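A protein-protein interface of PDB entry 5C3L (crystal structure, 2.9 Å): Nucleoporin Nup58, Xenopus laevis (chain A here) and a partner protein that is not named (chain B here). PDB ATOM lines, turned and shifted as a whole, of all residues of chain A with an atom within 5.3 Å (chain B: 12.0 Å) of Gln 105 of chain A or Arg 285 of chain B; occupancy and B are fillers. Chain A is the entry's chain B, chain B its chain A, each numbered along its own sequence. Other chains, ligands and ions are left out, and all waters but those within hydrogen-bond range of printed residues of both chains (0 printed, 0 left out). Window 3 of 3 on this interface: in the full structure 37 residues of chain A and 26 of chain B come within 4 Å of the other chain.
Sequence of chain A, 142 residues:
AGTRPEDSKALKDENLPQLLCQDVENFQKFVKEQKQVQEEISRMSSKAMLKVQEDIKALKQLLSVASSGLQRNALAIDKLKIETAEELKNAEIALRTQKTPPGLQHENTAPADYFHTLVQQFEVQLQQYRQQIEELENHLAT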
ATOM      1  N   THR A  97     -21.346 -11.232  33.240  1.00  0.00           N
ATOM      2  CA  THR A  97     -22.255 -10.306  32.565  1.00  0.00           C
ATOM      3  C   THR A  97     -23.342 -11.063  31.780  1.00  0.00           C
ATOM      4  O   THR A  97     -24.536 -10.803  31.943  1.00  0.00           O
ATOM      5  CB  THR A  97     -21.497  -9.370  31.600  1.00  0.00           C
ATOM      6  OG1 THR A  97     -20.497  -8.639  32.319  1.00  0.00           O
ATOM      7  CG2 THR A  97     -22.448  -8.383  30.926  1.00  0.00           C
ATOM      8  N   GLN A  98     -22.921 -12.003  30.939  1.00  0.00           N
ATOM      9  CA  GLN A  98     -23.846 -12.845  30.184  1.00  0.00           C
ATOM     10  C   GLN A  98     -24.864 -13.562  31.087  1.00  0.00           C
ATOM     11  O   GLN A  98     -26.055 -13.566  30.802  1.00  0.00           O
ATOM     12  CB  GLN A  98     -23.057 -13.876  29.363  1.00  0.00           C
ATOM     13  CG  GLN A  98     -23.909 -14.760  28.481  1.00  0.00           C
ATOM     14  CD  GLN A  98     -23.138 -15.329  27.304  1.00  0.00           C
ATOM     15  OE1 GLN A  98     -22.890 -16.533  27.233  1.00  0.00           O
ATOM     16  NE2 GLN A  98     -22.765 -14.461  26.360  1.00  0.00           N
ATOM     17  N   THR A 100     -25.965 -12.772  33.989  1.00  0.00           N
ATOM     18  CA  THR A 100     -26.862 -11.850  34.672  1.00  0.00           C
ATOM     19  C   THR A 100     -28.056 -11.524  33.799  1.00  0.00           C
ATOM     20  O   THR A 100     -27.872 -11.131  32.649  1.00  0.00           O
ATOM     21  CB  THR A 100     -26.136 -10.548  35.021  1.00  0.00           C
ATOM     22  OG1 THR A 100     -25.009 -10.841  35.865  1.00  0.00           O
ATOM     23  CG2 THR A 100     -27.104  -9.536  35.684  1.00  0.00           C
ATOM     24  N   PRO A 101     -29.281 -11.666  34.327  1.00  0.00           N
ATOM     25  CA  PRO A 101     -30.467 -11.286  33.542  1.00  0.00           C
ATOM     26  C   PRO A 101     -30.711  -9.781  33.503  1.00  0.00           C
ATOM     27  O   PRO A 101     -30.224  -9.080  34.382  1.00  0.00           O
ATOM     28  CB  PRO A 101     -31.605 -11.983  34.276  1.00  0.00           C
ATOM     29  CG  PRO A 101     -31.132 -12.042  35.711  1.00  0.00           C
ATOM     30  CD  PRO A 101     -29.649 -12.266  35.623  1.00  0.00           C
ATOM     31  N   PRO A 102     -31.479  -9.292  32.514  1.00  0.00           N
ATOM     32  CA  PRO A 102     -31.674  -7.845  32.311  1.00  0.00           C
ATOM     33  C   PRO A 102     -32.131  -7.099  33.561  1.00  0.00           C
ATOM     34  O   PRO A 102     -31.732  -5.955  33.763  1.00  0.00           O
ATOM     35  CB  PRO A 102     -32.741  -7.792  31.217  1.00  0.00           C
ATOM     36  CG  PRO A 102     -32.612  -9.123  30.490  1.00  0.00           C
ATOM     37  CD  PRO A 102     -32.274 -10.092  31.562  1.00  0.00           C
ATOM     38  N   GLY A 103     -32.918  -7.754  34.407  1.00  0.00           N
ATOM     39  CA  GLY A 103     -33.406  -7.146  35.638  1.00  0.00           C
ATOM     40  C   GLY A 103     -32.354  -6.911  36.712  1.00  0.00           C
ATOM     41  O   GLY A 103     -32.591  -6.154  37.645  1.00  0.00           O
ATOM     42  N   LEU A 104     -31.200  -7.552  36.588  1.00  0.00           N
ATOM     43  CA  LEU A 104     -30.113  -7.367  37.545  1.00  0.00           C
ATOM     44  C   LEU A 104     -28.831  -6.779  36.927  1.00  0.00           C
ATOM     45  O   LEU A 104     -27.759  -6.835  37.540  1.00  0.00           O
ATOM     46  CB  LEU A 104     -29.794  -8.706  38.210  1.00  0.00           C
ATOM     47  CG  LEU A 104     -30.909  -9.290  39.080  1.00  0.00           C
ATOM     48  CD1 LEU A 104     -30.554 -10.702  39.477  1.00  0.00           C
ATOM     49  CD2 LEU A 104     -31.157  -8.428  40.302  1.00  0.00           C
ATOM     50  N   GLN A 105     -28.929  -6.205  35.728  1.00  0.00           N
ATOM     51  CA  GLN A 105     -27.744  -5.669  35.054  1.00  0.00           C
ATOM     52  C   GLN A 105     -27.259  -4.356  35.698  1.00  0.00           C
ATOM     53  O   GLN A 105     -26.058  -4.067  35.694  1.00  0.00           O
ATOM     54  CB  GLN A 105     -28.026  -5.466  33.556  1.00  0.00           C
ATOM     55  CG  GLN A 105     -27.789  -6.731  32.705  1.00  0.00           C
ATOM     56  CD  GLN A 105     -26.316  -7.162  32.672  1.00  0.00           C
ATOM     57  OE1 GLN A 105     -25.409  -6.369  32.955  1.00  0.00           O
ATOM     58  NE2 GLN A 105     -26.081  -8.434  32.355  1.00  0.00           N
ATOM     59  N   HIS A 106     -28.182  -3.575  36.260  1.00  0.00           N
ATOM     60  CA  HIS A 106     -27.849  -2.308  36.918  1.00  0.00           C
ATOM     61  C   HIS A 106     -27.020  -2.534  38.175  1.00  0.00           C
ATOM     62  O   HIS A 106     -26.429  -1.597  38.721  1.00  0.00           O
ATOM     63  CB  HIS A 106     -29.124  -1.539  37.270  1.00  0.00           C
ATOM     64  CG  HIS A 106     -30.067  -2.306  38.147  1.00  0.00           C
ATOM     65  ND1 HIS A 106     -29.954  -2.334  39.521  1.00  0.00           N
ATOM     66  CD2 HIS A 106     -31.124  -3.095  37.842  1.00  0.00           C
ATOM     67  CE1 HIS A 106     -30.906  -3.098  40.022  1.00  0.00           C
ATOM     68  NE2 HIS A 106     -31.629  -3.574  39.026  1.00  0.00           N
ATOM     69  N   GLU A 107     -26.983  -3.782  38.626  1.00  0.00           N
ATOM     70  CA  GLU A 107     -26.182  -4.162  39.776  1.00  0.00           C
ATOM     71  C   GLU A 107     -24.888  -4.833  39.331  1.00  0.00           C
ATOM     72  O   GLU A 107     -24.098  -5.305  40.160  1.00  0.00           O
ATOM     73  CB  GLU A 107     -26.972  -5.092  40.695  1.00  0.00           C
ATOM     74  CG  GLU A 107     -28.014  -4.380  41.522  1.00  0.00           C
ATOM     75  CD  GLU A 107     -28.673  -5.293  42.526  1.00  0.00           C
ATOM     76  OE1 GLU A 107     -28.378  -6.507  42.500  1.00  0.00           O
ATOM     77  OE2 GLU A 107     -29.482  -4.799  43.342  1.00  0.00           O
ATOM     78  N   ASN A 108     -24.671  -4.861  38.018  1.00  0.00           N
ATOM     79  CA  ASN A 108     -23.437  -5.387  37.455  1.00  0.00           C
ATOM     80  C   ASN A 108     -22.422  -4.276  37.294  1.00  0.00           C
ATOM     81  O   ASN A 108     -22.256  -3.724  36.218  1.00  0.00           O
ATOM     82  CB  ASN A 108     -23.700  -6.061  36.116  1.00  0.00           C
ATOM     83  CG  ASN A 108     -22.496  -6.795  35.597  1.00  0.00           C
ATOM     84  OD1 ASN A 108     -21.502  -6.934  36.296  1.00  0.00           O
ATOM     85  ND2 ASN A 108     -22.583  -7.291  34.367  1.00  0.00           N
ATOM     86  N   THR A 109     -21.731  -3.973  38.383  1.00  0.00           N
ATOM     87  CA  THR A 109     -20.800  -2.860  38.436  1.00  0.00           C
ATOM     88  C   THR A 109     -19.380  -3.229  37.972  1.00  0.00           C
ATOM     89  O   THR A 109     -18.545  -2.347  37.745  1.00  0.00           O
ATOM     90  CB  THR A 109     -20.728  -2.311  39.871  1.00  0.00           C
ATOM     91  OG1 THR A 109     -20.200  -3.317  40.749  1.00  0.00           O
ATOM     92  CG2 THR A 109     -22.103  -1.904  40.333  1.00  0.00           C
ATOM     93  N   PRO A 111     -18.001  -4.553  35.138  1.00  0.00           N
ATOM     94  CA  PRO A 111     -17.550  -4.001  33.855  1.00  0.00           C
ATOM     95  C   PRO A 111     -17.119  -2.540  33.957  1.00  0.00           C
ATOM     96  O   PRO A 111     -16.180  -2.134  33.290  1.00  0.00           O
ATOM     97  CB  PRO A 111     -18.783  -4.133  32.958  1.00  0.00           C
ATOM     98  CG  PRO A 111     -19.576  -5.218  33.552  1.00  0.00           C
ATOM     99  CD  PRO A 111     -19.355  -5.119  35.034  1.00  0.00           C
ATOM    100  N   VAL B 274     -10.459 -10.247  25.033  1.00  0.00           N
ATOM    101  CA  VAL B 274     -11.354 -10.031  26.176  1.00  0.00           C
ATOM    102  C   VAL B 274     -11.901  -8.597  26.178  1.00  0.00           C
ATOM    103  O   VAL B 274     -13.092  -8.378  26.459  1.00  0.00           O
ATOM    104  CB  VAL B 274     -10.650 -10.299  27.535  1.00  0.00           C
ATOM    105  CG1 VAL B 274     -11.415  -9.624  28.707  1.00  0.00           C
ATOM    106  CG2 VAL B 274     -10.494 -11.799  27.775  1.00  0.00           C
ATOM    107  N   LEU B 275     -11.038  -7.624  25.882  1.00  0.00           N
ATOM    108  CA  LEU B 275     -11.468  -6.234  25.854  1.00  0.00           C
ATOM    109  C   LEU B 275     -12.524  -6.043  24.766  1.00  0.00           C
ATOM    110  O   LEU B 275     -13.399  -5.190  24.883  1.00  0.00           O
ATOM    111  CB  LEU B 275     -10.281  -5.293  25.622  1.00  0.00           C
ATOM    112  CG  LEU B 275     -10.652  -3.816  25.388  1.00  0.00           C
ATOM    113  CD1 LEU B 275     -11.375  -3.222  26.578  1.00  0.00           C
ATOM    114  CD2 LEU B 275      -9.433  -2.991  25.058  1.00  0.00           C
ATOM    115  N   GLN B 276     -12.451  -6.837  23.707  1.00  0.00           N
ATOM    116  CA  GLN B 276     -13.437  -6.737  22.647  1.00  0.00           C
ATOM    117  C   GLN B 276     -14.777  -7.296  23.100  1.00  0.00           C
ATOM    118  O   GLN B 276     -15.811  -6.702  22.823  1.00  0.00           O
ATOM    119  CB  GLN B 276     -12.941  -7.449  21.396  1.00  0.00           C
ATOM    120  CG  GLN B 276     -11.831  -6.669  20.707  1.00  0.00           C
ATOM    121  CD  GLN B 276     -11.111  -7.471  19.657  1.00  0.00           C
ATOM    122  OE1 GLN B 276     -11.019  -8.690  19.750  1.00  0.00           O
ATOM    123  NE2 GLN B 276     -10.605  -6.794  18.640  1.00  0.00           N
ATOM    124  N   VAL B 277     -14.766  -8.405  23.835  1.00  0.00           N
ATOM    125  CA  VAL B 277     -16.016  -8.972  24.336  1.00  0.00           C
ATOM    126  C   VAL B 277     -16.675  -8.054  25.358  1.00  0.00           C
ATOM    127  O   VAL B 277     -17.873  -7.773  25.257  1.00  0.00           O
ATOM    128  CB  VAL B 277     -15.810 -10.345  24.967  1.00  0.00           C
ATOM    129  CG1 VAL B 277     -17.112 -10.851  25.571  1.00  0.00           C
ATOM    130  CG2 VAL B 277     -15.324 -11.332  23.943  1.00  0.00           C
ATOM    131  N   LEU B 278     -15.909  -7.576  26.334  1.00  0.00           N
ATOM    132  CA  LEU B 278     -16.475  -6.688  27.337  1.00  0.00           C
ATOM    133  C   LEU B 278     -17.126  -5.488  26.639  1.00  0.00           C
ATOM    134  O   LEU B 278     -18.205  -5.066  27.027  1.00  0.00           O
ATOM    135  CB  LEU B 278     -15.408  -6.247  28.341  1.00  0.00           C
ATOM    136  CG  LEU B 278     -14.812  -7.426  29.117  1.00  0.00           C
ATOM    137  CD1 LEU B 278     -13.560  -6.994  29.851  1.00  0.00           C
ATOM    138  CD2 LEU B 278     -15.813  -8.066  30.076  1.00  0.00           C
ATOM    139  N   ILE B 279     -16.497  -4.990  25.577  1.00  0.00           N
ATOM    140  CA  ILE B 279     -17.008  -3.843  24.827  1.00  0.00           C
ATOM    141  C   ILE B 279     -18.348  -4.151  24.148  1.00  0.00           C
ATOM    142  O   ILE B 279     -19.321  -3.402  24.296  1.00  0.00           O
ATOM    143  CB  ILE B 279     -15.982  -3.397  23.759  1.00  0.00           C
ATOM    144  CG1 ILE B 279     -14.883  -2.553  24.413  1.00  0.00           C
ATOM    145  CG2 ILE B 279     -16.669  -2.648  22.612  1.00  0.00           C
ATOM    146  CD1 ILE B 279     -13.639  -2.408  23.574  1.00  0.00           C
ATOM    147  N   LYS B 280     -18.388  -5.243  23.391  1.00  0.00           N
ATOM    148  CA  LYS B 280     -19.624  -5.704  22.777  1.00  0.00           C
ATOM    149  C   LYS B 280     -20.751  -5.904  23.822  1.00  0.00           C
ATOM    150  O   LYS B 280     -21.895  -5.502  23.599  1.00  0.00           O
ATOM    151  CB  LYS B 280     -19.353  -6.998  22.010  1.00  0.00           C
ATOM    152  CG  LYS B 280     -18.496  -6.807  20.780  1.00  0.00           C
ATOM    153  CD  LYS B 280     -18.406  -8.084  19.974  1.00  0.00           C
ATOM    154  CE  LYS B 280     -17.581  -7.911  18.696  1.00  0.00           C
ATOM    155  NZ  LYS B 280     -16.110  -7.758  18.957  1.00  0.00           N
ATOM    156  N   GLN B 281     -20.427  -6.508  24.961  1.00  0.00           N
ATOM    157  CA  GLN B 281     -21.388  -6.645  26.057  1.00  0.00           C
ATOM    158  C   GLN B 281     -21.884  -5.288  26.545  1.00  0.00           C
ATOM    159  O   GLN B 281     -23.060  -5.129  26.822  1.00  0.00           O
ATOM    160  CB  GLN B 281     -20.771  -7.405  27.233  1.00  0.00           C
ATOM    161  CG  GLN B 281     -20.562  -8.900  27.014  1.00  0.00           C
ATOM    162  CD  GLN B 281     -19.802  -9.570  28.150  1.00  0.00           C
ATOM    163  OE1 GLN B 281     -18.948  -8.955  28.797  1.00  0.00           O
ATOM    164  NE2 GLN B 281     -20.109 -10.843  28.401  1.00  0.00           N
ATOM    165  N   GLU B 282     -20.998  -4.302  26.635  1.00  0.00           N
ATOM    166  CA  GLU B 282     -21.383  -3.027  27.228  1.00  0.00           C
ATOM    167  C   GLU B 282     -22.371  -2.356  26.302  1.00  0.00           C
ATOM    168  O   GLU B 282     -23.427  -1.905  26.740  1.00  0.00           O
ATOM    169  CB  GLU B 282     -20.179  -2.108  27.480  1.00  0.00           C
ATOM    170  CG  GLU B 282     -20.469  -0.985  28.484  1.00  0.00           C
ATOM    171  CD  GLU B 282     -20.687  -1.496  29.903  1.00  0.00           C
ATOM    172  OE1 GLU B 282     -20.414  -2.689  30.172  1.00  0.00           O
ATOM    173  OE2 GLU B 282     -21.125  -0.700  30.761  1.00  0.00           O
ATOM    174  N   ILE B 283     -22.044  -2.315  25.014  1.00  0.00           N
ATOM    175  CA  ILE B 283     -22.919  -1.674  24.034  1.00  0.00           C
ATOM    176  C   ILE B 283     -24.300  -2.343  24.008  1.00  0.00           C
ATOM    177  O   ILE B 283     -25.330  -1.667  24.022  1.00  0.00           O
ATOM    178  CB  ILE B 283     -22.305  -1.716  22.613  1.00  0.00           C
ATOM    179  CG1 ILE B 283     -20.952  -1.010  22.604  1.00  0.00           C
ATOM    180  CG2 ILE B 283     -23.248  -1.068  21.589  1.00  0.00           C
ATOM    181  CD1 ILE B 283     -20.163  -1.289  21.381  1.00  0.00           C
ATOM    182  N   GLN B 284     -24.304  -3.669  23.960  1.00  0.00           N
ATOM    183  CA  GLN B 284     -25.533  -4.436  23.939  1.00  0.00           C
ATOM    184  C   GLN B 284     -26.409  -4.196  25.193  1.00  0.00           C
ATOM    185  O   GLN B 284     -27.546  -3.743  25.093  1.00  0.00           O
ATOM    186  CB  GLN B 284     -25.185  -5.918  23.797  1.00  0.00           C
ATOM    187  CG  GLN B 284     -24.595  -6.300  22.450  1.00  0.00           C
ATOM    188  CD  GLN B 284     -24.065  -7.723  22.428  1.00  0.00           C
ATOM    189  OE1 GLN B 284     -24.396  -8.529  23.291  1.00  0.00           O
ATOM    190  NE2 GLN B 284     -23.235  -8.040  21.439  1.00  0.00           N
ATOM    191  N   ARG B 285     -25.879  -4.482  26.371  1.00  0.00           N
ATOM    192  CA  ARG B 285     -26.665  -4.398  27.589  1.00  0.00           C
ATOM    193  C   ARG B 285     -27.075  -2.970  27.959  1.00  0.00           C
ATOM    194  O   ARG B 285     -27.857  -2.775  28.884  1.00  0.00           O
ATOM    195  CB  ARG B 285     -25.879  -5.020  28.741  1.00  0.00           C
ATOM    196  CG  ARG B 285     -24.728  -4.177  29.224  1.00  0.00           C
ATOM    197  CD  ARG B 285     -23.835  -4.958  30.180  1.00  0.00           C
ATOM    198  NE  ARG B 285     -24.139  -4.617  31.568  1.00  0.00           N
ATOM    199  CZ  ARG B 285     -23.417  -3.796  32.325  1.00  0.00           C
ATOM    200  NH1 ARG B 285     -22.313  -3.234  31.854  1.00  0.00           N
ATOM    201  NH2 ARG B 285     -23.801  -3.545  33.567  1.00  0.00           N
ATOM    202  N   LYS B 286     -26.539  -1.982  27.255  1.00  0.00           N
ATOM    203  CA  LYS B 286     -26.908  -0.586  27.474  1.00  0.00           C
ATOM    204  C   LYS B 286     -27.693  -0.028  26.289  1.00  0.00           C
ATOM    205  O   LYS B 286     -27.780   1.185  26.126  1.00  0.00           O
ATOM    206  CB  LYS B 286     -25.668   0.273  27.710  1.00  0.00           C
ATOM    207  CG  LYS B 286     -24.966   0.020  29.013  1.00  0.00           C
ATOM    208  CD  LYS B 286     -25.205   1.142  30.003  1.00  0.00           C
ATOM    209  CE  LYS B 286     -24.041   1.287  30.961  1.00  0.00           C
ATOM    210  NZ  LYS B 286     -24.214   2.482  31.829  1.00  0.00           N
ATOM    211  N   SER B 287     -28.260  -0.914  25.470  1.00  0.00           N
ATOM    212  CA  SER B 287     -29.018  -0.513  24.282  1.00  0.00           C
ATOM    213  C   SER B 287     -30.170   0.427  24.599  1.00  0.00           C
ATOM    214  O   SER B 287     -31.045   0.102  25.401  1.00  0.00           O
ATOM    215  CB  SER B 287     -29.581  -1.737  23.560  1.00  0.00           C
ATOM    216  OG  SER B 287     -28.559  -2.480  22.918  1.00  0.00           O
ATOM    217  N   GLY B 288     -30.159   1.590  23.959  1.00  0.00           N
ATOM    218  CA  GLY B 288     -31.253   2.531  24.069  1.00  0.00           C
ATOM    219  C   GLY B 288     -31.258   3.291  25.375  1.00  0.00           C
ATOM    220  O   GLY B 288     -32.314   3.679  25.867  1.00  0.00           O
ATOM    221  N   PHE B 289     -30.074   3.509  25.934  1.00  0.00           N
ATOM    222  CA  PHE B 289     -29.928   4.304  27.146  1.00  0.00           C
ATOM    223  C   PHE B 289     -29.193   5.598  26.831  1.00  0.00           C
ATOM    224  O   PHE B 289     -28.347   5.637  25.940  1.00  0.00           O
ATOM    225  CB  PHE B 289     -29.183   3.517  28.236  1.00  0.00           C
ATOM    226  CG  PHE B 289     -29.997   2.408  28.860  1.00  0.00           C
ATOM    227  CD1 PHE B 289     -31.329   2.224  28.521  1.00  0.00           C
ATOM    228  CD2 PHE B 289     -29.436   1.557  29.799  1.00  0.00           C
ATOM    229  CE1 PHE B 289     -32.079   1.214  29.096  1.00  0.00           C
ATOM    230  CE2 PHE B 289     -30.184   0.541  30.375  1.00  0.00           C
ATOM    231  CZ  PHE B 289     -31.505   0.373  30.024  1.00  0.00           C
ATOM    232  N   ALA B 290     -29.537   6.654  27.563  1.00  0.00           N
ATOM    233  CA  ALA B 290     -28.865   7.939  27.436  1.00  0.00           C
ATOM    234  C   ALA B 290     -27.366   7.752  27.609  1.00  0.00           C
ATOM    235  O   ALA B 290     -26.925   6.887  28.363  1.00  0.00           O
ATOM    236  CB  ALA B 290     -29.399   8.925  28.458  1.00  0.00           C
ATOM    237  N   ILE B 291     -26.590   8.575  26.912  1.00  0.00           N
ATOM    238  CA  ILE B 291     -25.148   8.393  26.825  1.00  0.00           C
ATOM    239  C   ILE B 291     -24.507   8.347  28.208  1.00  0.00           C
ATOM    240  O   ILE B 291     -23.468   7.722  28.381  1.00  0.00           O
ATOM    241  CB  ILE B 291     -24.497   9.504  25.983  1.00  0.00           C
ATOM    242  CG1 ILE B 291     -25.236   9.657  24.646  1.00  0.00           C
ATOM    243  CG2 ILE B 291     -23.024   9.197  25.734  1.00  0.00           C
ATOM    244  CD1 ILE B 291     -26.158  10.873  24.563  1.00  0.00           C
ATOM    245  N   GLN B 292     -25.135   8.988  29.191  1.00  0.00           N
ATOM    246  CA  GLN B 292     -24.748   8.811  30.595  1.00  0.00           C
ATOM    247  C   GLN B 292     -23.409   9.472  30.954  1.00  0.00           C
ATOM    248  O   GLN B 292     -22.460   9.463  30.174  1.00  0.00           O
ATOM    249  CB  GLN B 292     -24.695   7.318  30.929  1.00  0.00           C
ATOM    250  CG  GLN B 292     -25.367   6.933  32.230  1.00  0.00           C
ATOM    251  CD  GLN B 292     -26.116   5.626  32.120  1.00  0.00           C
ATOM    252  OE1 GLN B 292     -25.605   4.571  32.486  1.00  0.00           O
ATOM    253  NE2 GLN B 292     -27.337   5.687  31.610  1.00  0.00           N
ATOM    254  N   GLU B 294     -20.770   9.153  33.381  1.00  0.00           N
ATOM    255  CA  GLU B 294     -19.485   8.495  33.573  1.00  0.00           C
ATOM    256  C   GLU B 294     -18.939   7.954  32.260  1.00  0.00           C
ATOM    257  O   GLU B 294     -17.734   7.721  32.129  1.00  0.00           O
ATOM    258  CB  GLU B 294     -19.611   7.366  34.596  1.00  0.00           C
ATOM    259  CG  GLU B 294     -20.736   6.390  34.293  1.00  0.00           C
ATOM    260  CD  GLU B 294     -20.415   4.962  34.707  1.00  0.00           C
ATOM    261  OE1 GLU B 294     -19.819   4.768  35.791  1.00  0.00           O
ATOM    262  OE2 GLU B 294     -20.757   4.034  33.939  1.00  0.00           O
ATOM    263  N   GLU B 295     -19.829   7.759  31.289  1.00  0.00           N
ATOM    264  CA  GLU B 295     -19.440   7.261  29.972  1.00  0.00           C
ATOM    265  C   GLU B 295     -18.803   8.370  29.136  1.00  0.00           C
ATOM    266  O   GLU B 295     -17.895   8.120  28.347  1.00  0.00           O
ATOM    267  CB  GLU B 295     -20.648   6.677  29.251  1.00  0.00           C
ATOM    268  CG  GLU B 295     -20.514   5.199  28.961  1.00  0.00           C
ATOM    269  CD  GLU B 295     -21.846   4.466  28.898  1.00  0.00           C
ATOM    270  OE1 GLU B 295     -22.875   5.084  28.521  1.00  0.00           O
ATOM    271  OE2 GLU B 295     -21.853   3.258  29.239  1.00  0.00           O
ATOM    272  N   LEU B 298     -15.106   9.013  30.155  1.00  0.00           N
ATOM    273  CA  LEU B 298     -14.133   8.156  29.492  1.00  0.00           C
ATOM    274  C   LEU B 298     -13.686   8.795  28.201  1.00  0.00           C
ATOM    275  O   LEU B 298     -12.487   8.895  27.927  1.00  0.00           O
ATOM    276  CB  LEU B 298     -14.714   6.784  29.175  1.00  0.00           C
ATOM    277  CG  LEU B 298     -14.806   5.733  30.269  1.00  0.00           C
ATOM    278  CD1 LEU B 298     -15.013   4.392  29.601  1.00  0.00           C
ATOM    279  CD2 LEU B 298     -13.582   5.707  31.194  1.00  0.00           C
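Of the 22 printed residues of chain B, 3 touch a printed residue of chain A. Hydrophobic or aromatic side chains of chain A within 4 Å of the printed part of chain B: Pro 111. Along chain A the printed residues that touch a printed residue of chain B span positions 97 to 111. Among the printed residues, 7 pairs touch across the chains. Among the printed residues, no Asp or Glu carboxylate lies within 4 Å of a Lys or Arg side-chain nitrogen of the other chain.
Thr 97 of chain A touches Gln 281 of chain B. Thr 97 of chain A touches Arg 285 of chain B (CG2 to CD, 3.8 Å). N of Gln 98 of chain A touches NE2 of Gln 281 of chain B, 3.96 Å away. CB of Pro 111 of chain A touches OE1 of Glu 282 of chain B (3.5 Å). Pro 111 of chain A touches Arg 285 of chain B (CG to NH1, 3.8 Å).
OE1 of Gln 105 of chain A lies within hydrogen-bond range of NE of Arg 285 of chain B. NH2 of Arg 285 of chain B sits at hydrogen-bond distance from O of Asn 108 of chain A (3.1 Å).
Of chain B, only Arg 285 comes within 4 Å of Gln 105 of chain A. Arg 285 of chain B touches just these residues of chain A: Thr 97 (3.8 Å), Gln 105 (2.6 Å), Asn 108 (3.1 Å) and Pro 111 (3.8 Å). Thr 97 of chain A touches two residues of chain B. No residue of chain B comes within 4 Å of Thr 100 of chain A. No residue of chain B comes within 4 Å of Pro 101 of chain A. No residue of chain B comes within 4 Å of His 106 of chain A. Glu 107 of chain A touches none of the printed residues of chain B. Asn 108 of chain A touches one residue of chain B. No residue of chain B comes within 4 Å of Thr 109 of chain A. Of chain B, only Glu 282 and Arg 285 come within 4 Å of Pro 111 of chain A. Of the printed residues of chain B, Gln 98 of chain A touches Gln 281. Printed residues of chain A within 4 Å of Glu 282 of chain B: Pro 111 (3.5 Å). Of the printed residues of chain A, Gln 281 of chain B touches Thr 97 (3.8 Å) and Gln 98 (3.96 Å). Val 274 of chain B touches none of the printed residues of chain A. Leu 298 of chain B touches none of the printed residues of chain A. The nearest residue of chain B that does not touch Gln 105 of chain A is Gln 281 of chain B (6.7 Å). The nearest printed residue of chain A that does not touch Gln 281 of chain B is Pro 111 of chain A (6.1 Å).
The guanidinium group of Arg 285 of chain B lies within salt-bridge range of the side-chain carboxylate of Glu 282 of chain B. NE2 of Gln 105 of chain A is in hydrogen-bond range of O of Thr 97 of chain A (2.9 Å). OG1 of Thr 97 of chain A is in hydrogen-bond range of ND2 of Asn 108 of chain A (3.2 Å). The backbone carbonyl oxygen (O) of Thr 100 of chain A is in hydrogen-bond range of the side-chain amide nitrogen (NE2) of Gln 105 of chain A, at 3.3 Å. OE1 of Gln 105 of chain A sits at hydrogen-bond distance from ND2 of Asn 108 of chain A (3.3 Å).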
